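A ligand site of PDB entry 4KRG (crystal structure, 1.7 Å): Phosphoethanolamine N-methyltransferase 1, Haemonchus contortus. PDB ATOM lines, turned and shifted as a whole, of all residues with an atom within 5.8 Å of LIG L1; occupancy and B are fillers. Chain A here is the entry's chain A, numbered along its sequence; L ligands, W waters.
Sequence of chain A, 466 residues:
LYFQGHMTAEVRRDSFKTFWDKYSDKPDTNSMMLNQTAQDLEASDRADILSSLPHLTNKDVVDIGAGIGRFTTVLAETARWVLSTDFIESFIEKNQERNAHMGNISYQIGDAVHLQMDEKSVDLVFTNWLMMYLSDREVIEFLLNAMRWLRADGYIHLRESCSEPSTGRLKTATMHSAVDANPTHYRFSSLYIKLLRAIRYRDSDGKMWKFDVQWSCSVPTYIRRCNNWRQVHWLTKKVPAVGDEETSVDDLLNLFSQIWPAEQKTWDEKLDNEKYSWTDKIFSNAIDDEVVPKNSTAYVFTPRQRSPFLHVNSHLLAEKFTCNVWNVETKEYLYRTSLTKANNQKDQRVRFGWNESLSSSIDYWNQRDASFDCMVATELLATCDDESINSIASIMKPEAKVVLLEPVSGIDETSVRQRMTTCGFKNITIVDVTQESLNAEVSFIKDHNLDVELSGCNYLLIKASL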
ATOM      1  N   ARG A  13     -14.703   7.862 -15.211  1.00  0.00           N
ATOM      2  CA  ARG A  13     -14.295   9.180 -15.640  1.00  0.00           C
ATOM      3  C   ARG A  13     -13.031   9.575 -14.890  1.00  0.00           C
ATOM      4  O   ARG A  13     -12.058  10.048 -15.493  1.00  0.00           O
ATOM      5  CB  ARG A  13     -15.400  10.211 -15.386  1.00  0.00           C
ATOM      6  CG  ARG A  13     -15.059  11.624 -15.830  1.00  0.00           C
ATOM      7  CD  ARG A  13     -15.570  11.952 -17.236  1.00  0.00           C
ATOM      8  NE  ARG A  13     -15.160  10.962 -18.229  1.00  0.00           N
ATOM      9  CZ  ARG A  13     -13.977  10.934 -18.822  1.00  0.00           C
ATOM     10  NH1 ARG A  13     -13.064  11.850 -18.537  1.00  0.00           N
ATOM     11  NH2 ARG A  13     -13.713   9.978 -19.711  1.00  0.00           N
ATOM     12  N   PHE A  16      -9.415   8.084 -15.722  1.00  0.00           N
ATOM     13  CA  PHE A  16      -8.665   8.731 -16.802  1.00  0.00           C
ATOM     14  C   PHE A  16      -7.958   9.983 -16.319  1.00  0.00           C
ATOM     15  O   PHE A  16      -6.796  10.208 -16.638  1.00  0.00           O
ATOM     16  CB  PHE A  16      -9.581   9.030 -17.997  1.00  0.00           C
ATOM     17  CG  PHE A  16      -9.868   7.830 -18.850  1.00  0.00           C
ATOM     18  CD1 PHE A  16      -8.856   7.199 -19.554  1.00  0.00           C
ATOM     19  CD2 PHE A  16     -11.159   7.334 -18.956  1.00  0.00           C
ATOM     20  CE1 PHE A  16      -9.120   6.087 -20.350  1.00  0.00           C
ATOM     21  CE2 PHE A  16     -11.435   6.218 -19.744  1.00  0.00           C
ATOM     22  CZ  PHE A  16     -10.416   5.600 -20.446  1.00  0.00           C
ATOM     23  N   TRP A  20      -3.913  10.653 -16.191  1.00  0.00           N
ATOM     24  CA  TRP A  20      -3.227  11.820 -16.728  1.00  0.00           C
ATOM     25  C   TRP A  20      -2.589  12.678 -15.646  1.00  0.00           C
ATOM     26  O   TRP A  20      -1.628  13.393 -15.913  1.00  0.00           O
ATOM     27  CB  TRP A  20      -4.146  12.618 -17.657  1.00  0.00           C
ATOM     28  CG  TRP A  20      -4.167  12.016 -19.027  1.00  0.00           C
ATOM     29  CD1 TRP A  20      -5.171  11.305 -19.598  1.00  0.00           C
ATOM     30  CD2 TRP A  20      -3.093  12.044 -19.959  1.00  0.00           C
ATOM     31  NE1 TRP A  20      -4.795  10.893 -20.852  1.00  0.00           N
ATOM     32  CE2 TRP A  20      -3.518  11.328 -21.107  1.00  0.00           C
ATOM     33  CE3 TRP A  20      -1.810  12.594 -19.962  1.00  0.00           C
ATOM     34  CZ2 TRP A  20      -2.706  11.168 -22.217  1.00  0.00           C
ATOM     35  CZ3 TRP A  20      -1.010  12.431 -21.064  1.00  0.00           C
ATOM     36  CH2 TRP A  20      -1.454  11.719 -22.186  1.00  0.00           C
ATOM     37  N   SER A  31       4.897  13.432 -22.753  1.00  0.00           N
ATOM     38  CA  SER A  31       3.612  13.052 -22.171  1.00  0.00           C
ATOM     39  C   SER A  31       2.473  13.064 -23.185  1.00  0.00           C
ATOM     40  O   SER A  31       1.622  12.165 -23.204  1.00  0.00           O
ATOM     41  CB  SER A  31       3.260  13.968 -20.997  1.00  0.00           C
ATOM     42  OG  SER A  31       4.061  13.648 -19.873  1.00  0.00           O
ATOM     43  N   MET A  32       2.465  14.096 -24.036  1.00  0.00           N
ATOM     44  CA  MET A  32       1.427  14.275 -25.047  1.00  0.00           C
ATOM     45  C   MET A  32       1.370  13.097 -25.977  1.00  0.00           C
ATOM     46  O   MET A  32       0.310  12.721 -26.469  1.00  0.00           O
ATOM     47  CB  MET A  32       1.708  15.541 -25.864  1.00  0.00           C
ATOM     48  CG  MET A  32       1.754  16.826 -25.048  1.00  0.00           C
ATOM     49  SD  MET A  32       0.122  17.113 -23.993  1.00  0.00           S
ATOM     50  CE  MET A  32       0.687  16.287 -22.323  1.00  0.00           C
ATOM     51  N   MET A  33       2.528  12.512 -26.238  1.00  0.00           N
ATOM     52  CA  MET A  33       2.614  11.421 -27.196  1.00  0.00           C
ATOM     53  C   MET A  33       2.872  10.105 -26.485  1.00  0.00           C
ATOM     54  O   MET A  33       2.859   9.053 -27.120  1.00  0.00           O
ATOM     55  CB  MET A  33       3.708  11.720 -28.215  1.00  0.00           C
ATOM     56  CG  MET A  33       3.573  13.110 -28.826  1.00  0.00           C
ATOM     57  SD  MET A  33       4.846  13.422 -30.277  1.00  0.00           S
ATOM     58  CE  MET A  33       3.801  12.721 -31.777  1.00  0.00           C
ATOM     59  N   ASP A  63     -10.169  23.287 -29.864  1.00  0.00           N
ATOM     60  CA  ASP A  63      -9.181  22.213 -29.758  1.00  0.00           C
ATOM     61  C   ASP A  63      -9.374  21.567 -28.391  1.00  0.00           C
ATOM     62  O   ASP A  63      -8.963  22.127 -27.378  1.00  0.00           O
ATOM     63  CB  ASP A  63      -7.763  22.771 -29.914  1.00  0.00           C
ATOM     64  CG  ASP A  63      -6.670  21.716 -29.740  1.00  0.00           C
ATOM     65  OD1 ASP A  63      -6.980  20.495 -29.617  1.00  0.00           O
ATOM     66  OD2 ASP A  63      -5.484  22.100 -29.723  1.00  0.00           O
ATOM     67  N   ILE A  64      -9.998  20.391 -28.389  1.00  0.00           N
ATOM     68  CA  ILE A  64     -10.405  19.736 -27.136  1.00  0.00           C
ATOM     69  C   ILE A  64      -9.430  18.625 -26.748  1.00  0.00           C
ATOM     70  O   ILE A  64      -9.177  17.712 -27.521  1.00  0.00           O
ATOM     71  CB  ILE A  64     -11.811  19.155 -27.280  1.00  0.00           C
ATOM     72  CG1 ILE A  64     -12.776  20.251 -27.730  1.00  0.00           C
ATOM     73  CG2 ILE A  64     -12.279  18.541 -25.964  1.00  0.00           C
ATOM     74  CD1 ILE A  64     -14.182  19.758 -27.967  1.00  0.00           C
ATOM     75  N   GLY A  65      -8.889  18.703 -25.535  1.00  0.00           N
ATOM     76  CA  GLY A  65      -7.833  17.792 -25.104  1.00  0.00           C
ATOM     77  C   GLY A  65      -6.506  18.267 -25.664  1.00  0.00           C
ATOM     78  O   GLY A  65      -5.633  17.483 -26.006  1.00  0.00           O
ATOM     79  N   ALA A  66      -6.368  19.591 -25.742  1.00  0.00           N
ATOM     80  CA  ALA A  66      -5.219  20.235 -26.386  1.00  0.00           C
ATOM     81  C   ALA A  66      -3.904  20.048 -25.631  1.00  0.00           C
ATOM     82  O   ALA A  66      -2.843  20.265 -26.202  1.00  0.00           O
ATOM     83  CB  ALA A  66      -5.501  21.717 -26.555  1.00  0.00           C
ATOM     84  N   GLY A  67      -3.990  19.680 -24.361  1.00  0.00           N
ATOM     85  CA  GLY A  67      -2.802  19.555 -23.525  1.00  0.00           C
ATOM     86  C   GLY A  67      -1.949  20.813 -23.546  1.00  0.00           C
ATOM     87  O   GLY A  67      -2.469  21.927 -23.474  1.00  0.00           O
ATOM     88  N   ILE A  68      -0.631  20.638 -23.689  1.00  0.00           N
ATOM     89  CA  ILE A  68       0.289  21.768 -23.698  1.00  0.00           C
ATOM     90  C   ILE A  68       0.163  22.606 -24.973  1.00  0.00           C
ATOM     91  O   ILE A  68       0.873  23.606 -25.140  1.00  0.00           O
ATOM     92  CB  ILE A  68       1.742  21.316 -23.521  1.00  0.00           C
ATOM     93  CG1 ILE A  68       2.190  20.451 -24.708  1.00  0.00           C
ATOM     94  CG2 ILE A  68       1.921  20.576 -22.191  1.00  0.00           C
ATOM     95  CD1 ILE A  68       3.664  20.053 -24.665  1.00  0.00           C
ATOM     96  N   ARG A  70       0.378  21.926 -28.510  1.00  0.00           N
ATOM     97  CA  ARG A  70       1.239  21.921 -29.693  1.00  0.00           C
ATOM     98  C   ARG A  70       0.478  22.136 -31.007  1.00  0.00           C
ATOM     99  O   ARG A  70       1.019  22.681 -31.962  1.00  0.00           O
ATOM    100  CB  ARG A  70       2.135  20.680 -29.743  1.00  0.00           C
ATOM    101  CG  ARG A  70       1.394  19.373 -29.723  1.00  0.00           C
ATOM    102  CD  ARG A  70       2.326  18.184 -29.530  1.00  0.00           C
ATOM    103  NE  ARG A  70       1.591  16.967 -29.828  1.00  0.00           N
ATOM    104  CZ  ARG A  70       1.626  16.309 -30.985  1.00  0.00           C
ATOM    105  NH1 ARG A  70       2.383  16.714 -31.989  1.00  0.00           N
ATOM    106  NH2 ARG A  70       0.882  15.229 -31.125  1.00  0.00           N
ATOM    107  N   PHE A  71      -0.790  21.739 -31.065  1.00  0.00           N
ATOM    108  CA  PHE A  71      -1.624  22.050 -32.218  1.00  0.00           C
ATOM    109  C   PHE A  71      -2.220  23.453 -32.099  1.00  0.00           C
ATOM    110  O   PHE A  71      -2.285  24.191 -33.092  1.00  0.00           O
ATOM    111  CB  PHE A  71      -2.728  21.017 -32.386  1.00  0.00           C
ATOM    112  CG  PHE A  71      -2.237  19.670 -32.813  1.00  0.00           C
ATOM    113  CD1 PHE A  71      -1.791  19.459 -34.109  1.00  0.00           C
ATOM    114  CD2 PHE A  71      -2.230  18.604 -31.925  1.00  0.00           C
ATOM    115  CE1 PHE A  71      -1.336  18.203 -34.502  1.00  0.00           C
ATOM    116  CE2 PHE A  71      -1.778  17.358 -32.318  1.00  0.00           C
ATOM    117  CZ  PHE A  71      -1.325  17.160 -33.611  1.00  0.00           C
ATOM    118  N   THR A  85      -8.842  23.557 -24.696  1.00  0.00           N
ATOM    119  CA  THR A  85      -9.287  22.974 -23.422  1.00  0.00           C
ATOM    120  C   THR A  85      -8.530  21.693 -23.075  1.00  0.00           C
ATOM    121  O   THR A  85      -8.095  20.957 -23.960  1.00  0.00           O
ATOM    122  CB  THR A  85     -10.787  22.640 -23.445  1.00  0.00           C
ATOM    123  OG1 THR A  85     -11.007  21.446 -24.199  1.00  0.00           O
ATOM    124  CG2 THR A  85     -11.601  23.770 -24.052  1.00  0.00           C
ATOM    125  N   ASP A  86      -8.375  21.429 -21.777  1.00  0.00           N
ATOM    126  CA  ASP A  86      -7.814  20.175 -21.297  1.00  0.00           C
ATOM    127  C   ASP A  86      -8.235  20.010 -19.844  1.00  0.00           C
ATOM    128  O   ASP A  86      -8.448  21.001 -19.145  1.00  0.00           O
ATOM    129  CB  ASP A  86      -6.280  20.190 -21.408  1.00  0.00           C
ATOM    130  CG  ASP A  86      -5.686  18.793 -21.444  1.00  0.00           C
ATOM    131  OD1 ASP A  86      -5.543  18.240 -22.562  1.00  0.00           O
ATOM    132  OD2 ASP A  86      -5.362  18.235 -20.368  1.00  0.00           O
ATOM    133  N   PHE A  87      -8.355  18.768 -19.369  1.00  0.00           N
ATOM    134  CA  PHE A  87      -8.764  18.577 -17.978  1.00  0.00           C
ATOM    135  C   PHE A  87      -7.593  18.513 -16.984  1.00  0.00           C
ATOM    136  O   PHE A  87      -7.801  18.435 -15.780  1.00  0.00           O
ATOM    137  CB  PHE A  87      -9.813  17.452 -17.813  1.00  0.00           C
ATOM    138  CG  PHE A  87      -9.288  16.051 -17.990  1.00  0.00           C
ATOM    139  CD1 PHE A  87     -10.055  14.979 -17.575  1.00  0.00           C
ATOM    140  CD2 PHE A  87      -8.048  15.798 -18.554  1.00  0.00           C
ATOM    141  CE1 PHE A  87      -9.606  13.689 -17.716  1.00  0.00           C
ATOM    142  CE2 PHE A  87      -7.586  14.501 -18.692  1.00  0.00           C
ATOM    143  CZ  PHE A  87      -8.368  13.446 -18.279  1.00  0.00           C
ATOM    144  N   ILE A  88      -6.372  18.577 -17.504  1.00  0.00           N
ATOM    145  CA  ILE A  88      -5.193  18.690 -16.653  1.00  0.00           C
ATOM    146  C   ILE A  88      -4.710  20.133 -16.583  1.00  0.00           C
ATOM    147  O   ILE A  88      -4.302  20.703 -17.588  1.00  0.00           O
ATOM    148  CB  ILE A  88      -4.046  17.786 -17.120  1.00  0.00           C
ATOM    149  CG1 ILE A  88      -4.468  16.314 -17.065  1.00  0.00           C
ATOM    150  CG2 ILE A  88      -2.834  18.023 -16.246  1.00  0.00           C
ATOM    151  CD1 ILE A  88      -4.862  15.846 -15.703  1.00  0.00           C
ATOM    152  N   PHE A  91      -1.128  21.327 -17.734  1.00  0.00           N
ATOM    153  CA  PHE A  91      -0.989  21.281 -19.186  1.00  0.00           C
ATOM    154  C   PHE A  91      -1.480  22.593 -19.787  1.00  0.00           C
ATOM    155  O   PHE A  91      -0.802  23.206 -20.609  1.00  0.00           O
ATOM    156  CB  PHE A  91      -1.742  20.084 -19.797  1.00  0.00           C
ATOM    157  CG  PHE A  91      -1.126  18.739 -19.460  1.00  0.00           C
ATOM    158  CD1 PHE A  91       0.106  18.647 -18.817  1.00  0.00           C
ATOM    159  CD2 PHE A  91      -1.790  17.566 -19.788  1.00  0.00           C
ATOM    160  CE1 PHE A  91       0.659  17.410 -18.523  1.00  0.00           C
ATOM    161  CE2 PHE A  91      -1.252  16.335 -19.487  1.00  0.00           C
ATOM    162  CZ  PHE A  91      -0.019  16.255 -18.863  1.00  0.00           C
ATOM    163  N   GLY A 110     -11.225  21.844 -18.006  1.00  0.00           N
ATOM    164  CA  GLY A 110     -12.434  21.085 -17.772  1.00  0.00           C
ATOM    165  C   GLY A 110     -12.441  19.779 -18.550  1.00  0.00           C
ATOM    166  O   GLY A 110     -11.638  19.576 -19.460  1.00  0.00           O
ATOM    167  N   ASP A 111     -13.356  18.895 -18.190  1.00  0.00           N
ATOM    168  CA  ASP A 111     -13.486  17.620 -18.869  1.00  0.00           C
ATOM    169  C   ASP A 111     -14.314  17.802 -20.141  1.00  0.00           C
ATOM    170  O   ASP A 111     -15.328  18.496 -20.133  1.00  0.00           O
ATOM    171  CB  ASP A 111     -14.147  16.600 -17.948  1.00  0.00           C
ATOM    172  CG  ASP A 111     -14.047  15.188 -18.455  1.00  0.00           C
ATOM    173  OD1 ASP A 111     -14.457  14.938 -19.606  1.00  0.00           O
ATOM    174  OD2 ASP A 111     -13.553  14.320 -17.707  1.00  0.00           O
ATOM    175  N   ALA A 112     -13.869  17.183 -21.226  1.00  0.00           N
ATOM    176  CA  ALA A 112     -14.569  17.238 -22.513  1.00  0.00           C
ATOM    177  C   ALA A 112     -16.006  16.708 -22.400  1.00  0.00           C
ATOM    178  O   ALA A 112     -16.905  17.127 -23.153  1.00  0.00           O
ATOM    179  CB  ALA A 112     -13.804  16.443 -23.555  1.00  0.00           C
ATOM    180  N   VAL A 113     -16.218  15.793 -21.463  1.00  0.00           N
ATOM    181  CA  VAL A 113     -17.547  15.228 -21.234  1.00  0.00           C
ATOM    182  C   VAL A 113     -18.559  16.288 -20.758  1.00  0.00           C
ATOM    183  O   VAL A 113     -19.753  16.187 -21.053  1.00  0.00           O
ATOM    184  CB  VAL A 113     -17.461  14.036 -20.260  1.00  0.00           C
ATOM    185  CG1 VAL A 113     -18.838  13.563 -19.836  1.00  0.00           C
ATOM    186  CG2 VAL A 113     -16.674  12.905 -20.901  1.00  0.00           C
ATOM    187  N   THR A 127      -9.644  17.480 -32.564  1.00  0.00           N
ATOM    188  CA  THR A 127      -9.122  16.618 -31.529  1.00  0.00           C
ATOM    189  C   THR A 127      -8.001  15.753 -32.101  1.00  0.00           C
ATOM    190  O   THR A 127      -7.908  15.566 -33.312  1.00  0.00           O
ATOM    191  CB  THR A 127     -10.217  15.700 -30.946  1.00  0.00           C
ATOM    192  OG1 THR A 127     -10.644  14.778 -31.944  1.00  0.00           O
ATOM    193  CG2 THR A 127     -11.406  16.515 -30.427  1.00  0.00           C
ATOM    194  N   ASN A 128      -7.174  15.232 -31.212  1.00  0.00           N
ATOM    195  CA  ASN A 128      -6.078  14.351 -31.596  1.00  0.00           C
ATOM    196  C   ASN A 128      -5.738  13.518 -30.363  1.00  0.00           C
ATOM    197  O   ASN A 128      -5.241  14.064 -29.373  1.00  0.00           O
ATOM    198  CB  ASN A 128      -4.871  15.163 -32.082  1.00  0.00           C
ATOM    199  CG  ASN A 128      -3.737  14.289 -32.611  1.00  0.00           C
ATOM    200  OD1 ASN A 128      -3.750  13.868 -33.771  1.00  0.00           O
ATOM    201  ND2 ASN A 128      -2.754  14.007 -31.760  1.00  0.00           N
ATOM    202  N   TRP A 129      -6.040  12.213 -30.414  1.00  0.00           N
ATOM    203  CA  TRP A 129      -5.934  11.303 -29.266  1.00  0.00           C
ATOM    204  C   TRP A 129      -6.905  11.631 -28.112  1.00  0.00           C
ATOM    205  O   TRP A 129      -6.457  12.001 -27.031  1.00  0.00           O
ATOM    206  CB  TRP A 129      -4.496  11.277 -28.701  1.00  0.00           C
ATOM    207  CG  TRP A 129      -3.455  10.589 -29.530  1.00  0.00           C
ATOM    208  CD1 TRP A 129      -3.568   9.402 -30.205  1.00  0.00           C
ATOM    209  CD2 TRP A 129      -2.122  11.049 -29.738  1.00  0.00           C
ATOM    210  NE1 TRP A 129      -2.374   9.096 -30.818  1.00  0.00           N
ATOM    211  CE2 TRP A 129      -1.467  10.084 -30.547  1.00  0.00           C
ATOM    212  CE3 TRP A 129      -1.393  12.175 -29.318  1.00  0.00           C
ATOM    213  CZ2 TRP A 129      -0.132  10.229 -30.938  1.00  0.00           C
ATOM    214  CZ3 TRP A 129      -0.086  12.301 -29.707  1.00  0.00           C
ATOM    215  CH2 TRP A 129       0.536  11.335 -30.513  1.00  0.00           C
ATOM    216  N   LEU A 130      -8.201  11.474 -28.324  1.00  0.00           N
ATOM    217  CA  LEU A 130      -9.168  11.809 -27.272  1.00  0.00           C
ATOM    218  C   LEU A 130     -10.267  10.760 -27.047  1.00  0.00           C
ATOM    219  O   LEU A 130     -10.559  10.407 -25.907  1.00  0.00           O
ATOM    220  CB  LEU A 130      -9.800  13.186 -27.506  1.00  0.00           C
ATOM    221  CG  LEU A 130     -10.762  13.646 -26.406  1.00  0.00           C
ATOM    222  CD1 LEU A 130     -10.033  13.818 -25.075  1.00  0.00           C
ATOM    223  CD2 LEU A 130     -11.465  14.935 -26.802  1.00  0.00           C
ATOM    224  N   TYR A 133      -9.844   7.923 -24.740  1.00  0.00           N
ATOM    225  CA  TYR A 133      -9.908   8.203 -23.305  1.00  0.00           C
ATOM    226  C   TYR A 133     -11.342   8.463 -22.827  1.00  0.00           C
ATOM    227  O   TYR A 133     -11.555   8.975 -21.730  1.00  0.00           O
ATOM    228  CB  TYR A 133      -8.999   9.386 -22.938  1.00  0.00           C
ATOM    229  CG  TYR A 133      -7.541   9.181 -23.320  1.00  0.00           C
ATOM    230  CD1 TYR A 133      -6.789   8.170 -22.735  1.00  0.00           C
ATOM    231  CD2 TYR A 133      -6.932   9.999 -24.268  1.00  0.00           C
ATOM    232  CE1 TYR A 133      -5.465   7.985 -23.085  1.00  0.00           C
ATOM    233  CE2 TYR A 133      -5.605   9.815 -24.628  1.00  0.00           C
ATOM    234  CZ  TYR A 133      -4.876   8.796 -24.028  1.00  0.00           C
ATOM    235  OH  TYR A 133      -3.559   8.599 -24.381  1.00  0.00           O
ATOM    236  N   LEU A 134     -12.313   8.100 -23.659  1.00  0.00           N
ATOM    237  CA  LEU A 134     -13.728   8.194 -23.311  1.00  0.00           C
ATOM    238  C   LEU A 134     -14.390   6.822 -23.393  1.00  0.00           C
ATOM    239  O   LEU A 134     -13.916   5.965 -24.128  1.00  0.00           O
ATOM    240  CB  LEU A 134     -14.463   9.154 -24.260  1.00  0.00           C
ATOM    241  CG  LEU A 134     -13.985  10.600 -24.295  1.00  0.00           C
ATOM    242  CD1 LEU A 134     -14.799  11.423 -25.279  1.00  0.00           C
ATOM    243  CD2 LEU A 134     -14.064  11.214 -22.926  1.00  0.00           C
HETATM  244  N1  LIG L   1      -4.115  16.324 -28.195  1.00  0.00           N
HETATM  245  C1  LIG L   1      -2.787  16.664 -27.664  1.00  0.00           C
HETATM  246  C2  LIG L   1      -2.535  15.822 -26.370  1.00  0.00           C
HETATM  247  C3  LIG L   1      -2.696  14.317 -26.567  1.00  0.00           C
HETATM  248  S1  LIG L   1      -2.643  13.320 -25.049  1.00  0.00           S
HETATM  249  C4  LIG L   1      -1.732  16.428 -28.673  1.00  0.00           C
HETATM  250  O1  LIG L   1      -1.840  15.510 -29.460  1.00  0.00           O
HETATM  251  O2  LIG L   1      -0.648  16.941 -28.500  1.00  0.00           O
HETATM  252  C5  LIG L   1      -4.297  13.500 -24.312  1.00  0.00           C
HETATM  253  C6  LIG L   1      -4.723  14.783 -23.857  1.00  0.00           C
HETATM  254  O3  LIG L   1      -6.172  14.804 -23.742  1.00  0.00           O
HETATM  255  C7  LIG L   1      -4.198  15.091 -22.516  1.00  0.00           C
HETATM  256  O4  LIG L   1      -3.869  16.465 -22.440  1.00  0.00           O
HETATM  257  C8  LIG L   1      -5.308  14.813 -21.622  1.00  0.00           C
HETATM  258  O5  LIG L   1      -5.226  15.580 -20.456  1.00  0.00           O
HETATM  259  C9  LIG L   1      -6.484  15.182 -22.447  1.00  0.00           C
HETATM  260  N2  LIG L   1      -7.770  14.526 -22.002  1.00  0.00           N
HETATM  261  C10 LIG L   1      -8.039  13.215 -21.933  1.00  0.00           C
HETATM  262  N3  LIG L   1      -9.335  13.096 -21.633  1.00  0.00           N
HETATM  263  C11 LIG L   1      -9.884  14.305 -21.516  1.00  0.00           C
HETATM  264  C12 LIG L   1     -11.177  14.763 -21.219  1.00  0.00           C
HETATM  265  N4  LIG L   1     -12.203  13.882 -20.967  1.00  0.00           N
HETATM  266  N5  LIG L   1     -11.393  16.088 -21.184  1.00  0.00           N
HETATM  267  C13 LIG L   1     -10.420  16.963 -21.429  1.00  0.00           C
HETATM  268  N6  LIG L   1      -9.166  16.555 -21.718  1.00  0.00           N
HETATM  269  C14 LIG L   1      -8.875  15.244 -21.765  1.00  0.00           C
HETATM  270  C1  LG2 L   2      -0.511   8.081 -27.342  1.00  0.00           C
HETATM  271  C2  LG2 L   2      -0.503   9.459 -26.762  1.00  0.00           C
HETATM  272  O1  LG2 L   2       0.470   5.402 -26.984  1.00  0.00           O
HETATM  273  O2  LG2 L   2      -1.671   5.229 -28.153  1.00  0.00           O
HETATM  274  O3  LG2 L   2      -1.605   4.852 -25.690  1.00  0.00           O
HETATM  275  O4  LG2 L   2      -1.249   7.152 -26.634  1.00  0.00           O
HETATM  276  N1  LG2 L   2      -1.769  10.051 -26.432  1.00  0.00           N
HETATM  277  P1  LG2 L   2      -1.018   5.620 -26.856  1.00  0.00           P
HETATM  278  O   HOH W   1      -0.520  19.203 -27.217  1.00  0.00           O
HETATM  279  O   HOH W   2     -10.966  11.274 -20.240  1.00  0.00           O
HETATM  280  O   HOH W   3      -5.208  18.536 -29.617  1.00  0.00           O
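The side-chain carboxylate (OD1) of Asp 86 sits at hydrogen-bond distance from an oxygen (O4) of LIG L1. The guanidinium group (NE) of Arg 70 lies within salt-bridge range of an oxygen (O2) of LIG L1 (2.6 Å). The backbone NH (N) of Ala 112 is in hydrogen-bond range of a nitrogen (N5) of LIG L1, at 2.7 Å. N1 of LIG L1 is in hydrogen-bond range of O of Asn 128 (2.8 Å). An oxygen (O1) of LIG L1 sits at hydrogen-bond distance from the side-chain amide nitrogen (ND2) of Asn 128, at 2.9 Å. OD1 of Asp 111 is in hydrogen-bond range of N4 of LIG L1 (2.8 Å). O of Gly 65 is in hydrogen-bond range of N1 of LIG L1, 2.9 Å away. The backbone NH (N) of Phe 87 is in hydrogen-bond range of a nitrogen (N6) of LIG L1. N1 of LG2 L2 sits close to O of Met 32. OH of Tyr 133 is in hydrogen-bond range of N1 of LG2 L2.
N of Gly 67 sits at hydrogen-bond distance from OD1 of Asp 86, at 2.8 Å. N of Ile 88 is in hydrogen-bond range of OD2 of Asp 86 (3.1 Å). The guanidinium group (NH1) of Arg 13 is in salt-bridge range of the side-chain carboxylate (OD2) of Asp 111, 2.7 Å away. N of Val 113 sits at hydrogen-bond distance from OD1 of Asp 111 (2.7 Å). N of Gly 65 lies within hydrogen-bond range of O of Thr 85 (2.9 Å). The backbone NH of Phe 87 sits close to the backbone carbonyl oxygen of Gly 110 (3.4 Å). O of Tyr 133 sits at hydrogen-bond distance from NH2 of Arg 13. The backbone NH of Ile 68 sits at hydrogen-bond distance from the side-chain sulfur of Met 32, at 3.6 Å.
Water W1 lies within hydrogen-bond range of O2 of LIG L1, O of Ala 66 and N of Arg 70. Water W2 lies within hydrogen-bond range of the guanidinium group (NH1) of Arg 13, the backbone carbonyl oxygen (O) of Tyr 133 and a nitrogen (N3) of LIG L1. Water W3 bridges the side-chain carboxylate of Asp 63 (2.6 Å) and a nitrogen (N1) of LIG L1 (2.8 Å).
N4 of LIG L1 lies close to NH1 of Arg 13 (3.3 Å). The backbone carbonyl oxygen (O) of Met 32 lies close to a sulfur (S1) of LIG L1 (3.3 Å). CH2 of Trp 20 touches S1 of LIG L1, at 3.5 Å. Ala 66 touches LIG L1 (O to C1, 3.9 Å). CA of Gly 67 touches O4 of LIG L1, at 3.4 Å. Phe 71 touches LIG L1. Ile 88 touches LIG L1. CD2 of Phe 91 touches O4 of LIG L1, 3.5 Å away. Gly 110 touches LIG L1 (O to C13, 3.5 Å). Trp 129 touches LIG L1. CD1 of Leu 130 touches N3 of LIG L1 (3.6 Å). Tyr 133 touches LIG L1 (CE2 to C5, 3.9 Å). Leu 134 touches LIG L1 (CD2 to N4, 3.8 Å). Hydrophobic or aromatic side chains within 4 Å of LIG L1: Trp 20, Met 32, Phe 71, Phe 87, Ile 88, Phe 91, Ala 112, Trp 129, Leu 130, Tyr 133 and Leu 134. Of the 29 residues printed, 20 come within 4 Å of LIG L1. The nearest printed residue that does not touch LIG L1 is Val 113 (4.5 Å).
S1 of LIG L1 sits close to N1 of LG2 L2 (3.7 Å).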
